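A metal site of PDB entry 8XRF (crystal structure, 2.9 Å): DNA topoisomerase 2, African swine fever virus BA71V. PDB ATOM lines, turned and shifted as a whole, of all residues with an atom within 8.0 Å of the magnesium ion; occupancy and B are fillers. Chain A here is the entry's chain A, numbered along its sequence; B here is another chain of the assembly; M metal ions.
The backbone carbonyl oxygen of Ala 664 of chain B is in hydrogen-bond range of the side-chain amide nitrogen of Asn 667 of chain B, at 3.3 Å.
O of Asn 667 of chain A lies within hydrogen-bond range of ND1 of His 670 of chain A.
ND2 of Asn 667 of chain A lies within hydrogen-bond range of O of Glu 665 of chain A, at 3.4 Å.
Of the 18 residues printed, 4 come within 4 Å of the magnesium ion.
The magnesium ion is bound by OD1 of Asn 667 of chain B (2.0 Å), OD1 of Asn 667 of chain A (2.1 Å) and O of Ala 664 of chain A (2.5 Å).
Slightly farther from the magnesium ion lies the backbone carbonyl oxygen (O) of Ala 664 of chain B (2.6 Å).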
ATOM      1  N   GLU A 662      26.972  30.698   0.380  1.00  0.00           N
ATOM      2  CA  GLU A 662      28.233  30.106  -0.050  1.00  0.00           C
ATOM      3  C   GLU A 662      28.045  28.724  -0.679  1.00  0.00           C
ATOM      4  O   GLU A 662      29.035  28.076  -1.028  1.00  0.00           O
ATOM      5  CB  GLU A 662      29.201  30.001   1.122  1.00  0.00           C
ATOM      6  CG  GLU A 662      29.898  31.299   1.502  1.00  0.00           C
ATOM      7  CD  GLU A 662      31.376  31.108   1.773  1.00  0.00           C
ATOM      8  OE1 GLU A 662      32.129  30.901   0.799  1.00  0.00           O
ATOM      9  OE2 GLU A 662      31.778  31.163   2.945  1.00  0.00           O
ATOM     10  N   SER A 663      26.801  28.272  -0.861  1.00  0.00           N
ATOM     11  CA  SER A 663      26.597  26.906  -1.335  1.00  0.00           C
ATOM     12  C   SER A 663      26.985  26.754  -2.806  1.00  0.00           C
ATOM     13  O   SER A 663      27.426  25.670  -3.211  1.00  0.00           O
ATOM     14  CB  SER A 663      25.132  26.500  -1.137  1.00  0.00           C
ATOM     15  OG  SER A 663      24.258  27.369  -1.822  1.00  0.00           O
ATOM     16  N   ALA A 664      26.834  27.804  -3.606  1.00  0.00           N
ATOM     17  CA  ALA A 664      27.113  27.691  -5.039  1.00  0.00           C
ATOM     18  C   ALA A 664      28.610  27.539  -5.298  1.00  0.00           C
ATOM     19  O   ALA A 664      29.021  26.669  -6.064  1.00  0.00           O
ATOM     20  CB  ALA A 664      26.562  28.905  -5.773  1.00  0.00           C
ATOM     21  N   GLU A 665      29.437  28.386  -4.670  1.00  0.00           N
ATOM     22  CA  GLU A 665      30.876  28.268  -4.867  1.00  0.00           C
ATOM     23  C   GLU A 665      31.437  27.074  -4.116  1.00  0.00           C
ATOM     24  O   GLU A 665      32.287  26.349  -4.635  1.00  0.00           O
ATOM     25  CB  GLU A 665      31.561  29.556  -4.397  1.00  0.00           C
ATOM     26  CG  GLU A 665      30.855  30.841  -4.821  1.00  0.00           C
ATOM     27  CD  GLU A 665      30.207  31.559  -3.651  1.00  0.00           C
ATOM     28  OE1 GLU A 665      29.380  30.929  -2.955  1.00  0.00           O
ATOM     29  OE2 GLU A 665      30.516  32.754  -3.432  1.00  0.00           O
ATOM     30  N   LEU A 666      30.963  26.861  -2.886  1.00  0.00           N
ATOM     31  CA  LEU A 666      31.447  25.781  -2.015  1.00  0.00           C
ATOM     32  C   LEU A 666      30.623  24.521  -2.286  1.00  0.00           C
ATOM     33  O   LEU A 666      29.791  24.084  -1.489  1.00  0.00           O
ATOM     34  CB  LEU A 666      31.374  26.223  -0.556  1.00  0.00           C
ATOM     35  CG  LEU A 666      32.066  25.569   0.625  1.00  0.00           C
ATOM     36  CD1 LEU A 666      32.359  26.650   1.655  1.00  0.00           C
ATOM     37  CD2 LEU A 666      31.191  24.493   1.251  1.00  0.00           C
ATOM     38  N   ASN A 667      30.870  23.930  -3.462  1.00  0.00           N
ATOM     39  CA  ASN A 667      30.077  22.807  -3.952  1.00  0.00           C
ATOM     40  C   ASN A 667      30.345  21.561  -3.122  1.00  0.00           C
ATOM     41  O   ASN A 667      31.405  20.946  -3.233  1.00  0.00           O
ATOM     42  CB  ASN A 667      30.380  22.554  -5.430  1.00  0.00           C
ATOM     43  CG  ASN A 667      29.915  23.680  -6.331  1.00  0.00           C
ATOM     44  OD1 ASN A 667      28.719  23.958  -6.433  1.00  0.00           O
ATOM     45  ND2 ASN A 667      30.868  24.337  -6.989  1.00  0.00           N
ATOM     46  N   LEU A 668      29.380  21.197  -2.280  1.00  0.00           N
ATOM     47  CA  LEU A 668      29.491  19.991  -1.458  1.00  0.00           C
ATOM     48  C   LEU A 668      29.561  18.707  -2.283  1.00  0.00           C
ATOM     49  O   LEU A 668      29.980  17.674  -1.763  1.00  0.00           O
ATOM     50  CB  LEU A 668      28.315  19.901  -0.496  1.00  0.00           C
ATOM     51  CG  LEU A 668      28.632  19.978   0.995  1.00  0.00           C
ATOM     52  CD1 LEU A 668      27.377  19.797   1.841  1.00  0.00           C
ATOM     53  CD2 LEU A 668      29.708  18.982   1.376  1.00  0.00           C
ATOM     54  N   SER A 669      29.130  18.758  -3.555  1.00  0.00           N
ATOM     55  CA  SER A 669      29.143  17.571  -4.405  1.00  0.00           C
ATOM     56  C   SER A 669      30.501  16.879  -4.462  1.00  0.00           C
ATOM     57  O   SER A 669      30.574  15.660  -4.597  1.00  0.00           O
ATOM     58  CB  SER A 669      28.703  17.944  -5.827  1.00  0.00           C
ATOM     59  OG  SER A 669      27.520  18.729  -5.807  1.00  0.00           O
ATOM     60  N   HIS A 670      31.599  17.649  -4.358  1.00  0.00           N
ATOM     61  CA  HIS A 670      32.936  17.107  -4.574  1.00  0.00           C
ATOM     62  C   HIS A 670      33.539  16.429  -3.359  1.00  0.00           C
ATOM     63  O   HIS A 670      34.542  15.728  -3.498  1.00  0.00           O
ATOM     64  CB  HIS A 670      33.903  18.196  -5.043  1.00  0.00           C
ATOM     65  CG  HIS A 670      33.427  18.972  -6.223  1.00  0.00           C
ATOM     66  ND1 HIS A 670      32.454  19.938  -6.128  1.00  0.00           N
ATOM     67  CD2 HIS A 670      33.774  18.912  -7.523  1.00  0.00           C
ATOM     68  CE1 HIS A 670      32.227  20.454  -7.326  1.00  0.00           C
ATOM     69  NE2 HIS A 670      33.016  19.847  -8.190  1.00  0.00           N
ATOM     70  N   GLU B 662      25.109  16.286 -11.490  1.00  0.00           N
ATOM     71  CA  GLU B 662      24.823  17.552 -12.143  1.00  0.00           C
ATOM     72  C   GLU B 662      24.496  18.666 -11.141  1.00  0.00           C
ATOM     73  O   GLU B 662      24.075  19.751 -11.544  1.00  0.00           O
ATOM     74  CB  GLU B 662      23.669  17.395 -13.139  1.00  0.00           C
ATOM     75  CG  GLU B 662      24.092  16.794 -14.476  1.00  0.00           C
ATOM     76  CD  GLU B 662      22.927  16.406 -15.362  1.00  0.00           C
ATOM     77  OE1 GLU B 662      21.928  17.161 -15.387  1.00  0.00           O
ATOM     78  OE2 GLU B 662      23.010  15.358 -16.030  1.00  0.00           O
ATOM     79  N   SER B 663      24.684  18.407  -9.844  1.00  0.00           N
ATOM     80  CA  SER B 663      24.295  19.369  -8.824  1.00  0.00           C
ATOM     81  C   SER B 663      25.200  20.593  -8.817  1.00  0.00           C
ATOM     82  O   SER B 663      24.757  21.692  -8.454  1.00  0.00           O
ATOM     83  CB  SER B 663      24.304  18.708  -7.443  1.00  0.00           C
ATOM     84  OG  SER B 663      25.612  18.295  -7.088  1.00  0.00           O
ATOM     85  N   ALA B 664      26.466  20.440  -9.204  1.00  0.00           N
ATOM     86  CA  ALA B 664      27.411  21.554  -9.122  1.00  0.00           C
ATOM     87  C   ALA B 664      27.063  22.643 -10.129  1.00  0.00           C
ATOM     88  O   ALA B 664      27.060  23.832  -9.784  1.00  0.00           O
ATOM     89  CB  ALA B 664      28.833  21.049  -9.360  1.00  0.00           C
ATOM     90  N   GLU B 665      26.774  22.271 -11.372  1.00  0.00           N
ATOM     91  CA  GLU B 665      26.399  23.263 -12.375  1.00  0.00           C
ATOM     92  C   GLU B 665      25.000  23.816 -12.126  1.00  0.00           C
ATOM     93  O   GLU B 665      24.759  25.007 -12.322  1.00  0.00           O
ATOM     94  CB  GLU B 665      26.505  22.668 -13.787  1.00  0.00           C
ATOM     95  CG  GLU B 665      26.173  21.195 -13.878  1.00  0.00           C
ATOM     96  CD  GLU B 665      26.138  20.709 -15.317  1.00  0.00           C
ATOM     97  OE1 GLU B 665      26.245  21.551 -16.225  1.00  0.00           O
ATOM     98  OE2 GLU B 665      26.001  19.481 -15.522  1.00  0.00           O
ATOM     99  N   LEU B 666      24.072  22.962 -11.692  1.00  0.00           N
ATOM    100  CA  LEU B 666      22.687  23.367 -11.485  1.00  0.00           C
ATOM    101  C   LEU B 666      22.555  23.994 -10.097  1.00  0.00           C
ATOM    102  O   LEU B 666      21.976  23.422  -9.164  1.00  0.00           O
ATOM    103  CB  LEU B 666      21.747  22.166 -11.629  1.00  0.00           C
ATOM    104  CG  LEU B 666      21.224  21.765 -12.997  1.00  0.00           C
ATOM    105  CD1 LEU B 666      22.320  21.137 -13.835  1.00  0.00           C
ATOM    106  CD2 LEU B 666      20.047  20.808 -12.841  1.00  0.00           C
ATOM    107  N   ASN B 667      23.103  25.197  -9.967  1.00  0.00           N
ATOM    108  CA  ASN B 667      23.147  25.861  -8.678  1.00  0.00           C
ATOM    109  C   ASN B 667      21.742  26.275  -8.293  1.00  0.00           C
ATOM    110  O   ASN B 667      21.233  27.296  -8.756  1.00  0.00           O
ATOM    111  CB  ASN B 667      24.081  27.074  -8.734  1.00  0.00           C
ATOM    112  CG  ASN B 667      25.544  26.694  -8.769  1.00  0.00           C
ATOM    113  OD1 ASN B 667      26.061  26.071  -7.845  1.00  0.00           O
ATOM    114  ND2 ASN B 667      26.229  27.065  -9.850  1.00  0.00           N
ATOM    115  N   LEU B 668      21.097  25.483  -7.433  1.00  0.00           N
ATOM    116  CA  LEU B 668      19.781  25.856  -6.929  1.00  0.00           C
ATOM    117  C   LEU B 668      19.842  27.114  -6.088  1.00  0.00           C
ATOM    118  O   LEU B 668      18.819  27.781  -5.898  1.00  0.00           O
ATOM    119  CB  LEU B 668      19.171  24.708  -6.131  1.00  0.00           C
ATOM    120  CG  LEU B 668      18.849  23.442  -6.918  1.00  0.00           C
ATOM    121  CD1 LEU B 668      18.125  22.428  -6.051  1.00  0.00           C
ATOM    122  CD2 LEU B 668      18.036  23.772  -8.157  1.00  0.00           C
ATOM    123  N   SER B 669      21.028  27.444  -5.560  1.00  0.00           N
ATOM    124  CA  SER B 669      21.209  28.659  -4.783  1.00  0.00           C
ATOM    125  C   SER B 669      20.759  29.897  -5.544  1.00  0.00           C
ATOM    126  O   SER B 669      20.291  30.863  -4.922  1.00  0.00           O
ATOM    127  CB  SER B 669      22.686  28.806  -4.376  1.00  0.00           C
ATOM    128  OG  SER B 669      23.293  27.538  -4.236  1.00  0.00           O
ATOM    129  N   HIS B 670      20.906  29.913  -6.870  1.00  0.00           N
ATOM    130  CA  HIS B 670      20.630  31.116  -7.641  1.00  0.00           C
ATOM    131  C   HIS B 670      19.163  31.262  -8.043  1.00  0.00           C
ATOM    132  O   HIS B 670      18.719  32.373  -8.311  1.00  0.00           O
ATOM    133  CB  HIS B 670      21.483  31.120  -8.917  1.00  0.00           C
ATOM    134  CG  HIS B 670      22.959  31.122  -8.653  1.00  0.00           C
ATOM    135  ND1 HIS B 670      23.504  31.456  -7.429  1.00  0.00           N
ATOM    136  CD2 HIS B 670      24.006  30.819  -9.455  1.00  0.00           C
ATOM    137  CE1 HIS B 670      24.817  31.369  -7.484  1.00  0.00           C
ATOM    138  NE2 HIS B 670      25.158  30.983  -8.704  1.00  0.00           N
HETATM  139 MG    MG M   1      27.957  25.332  -7.822  1.00  0.00          MG
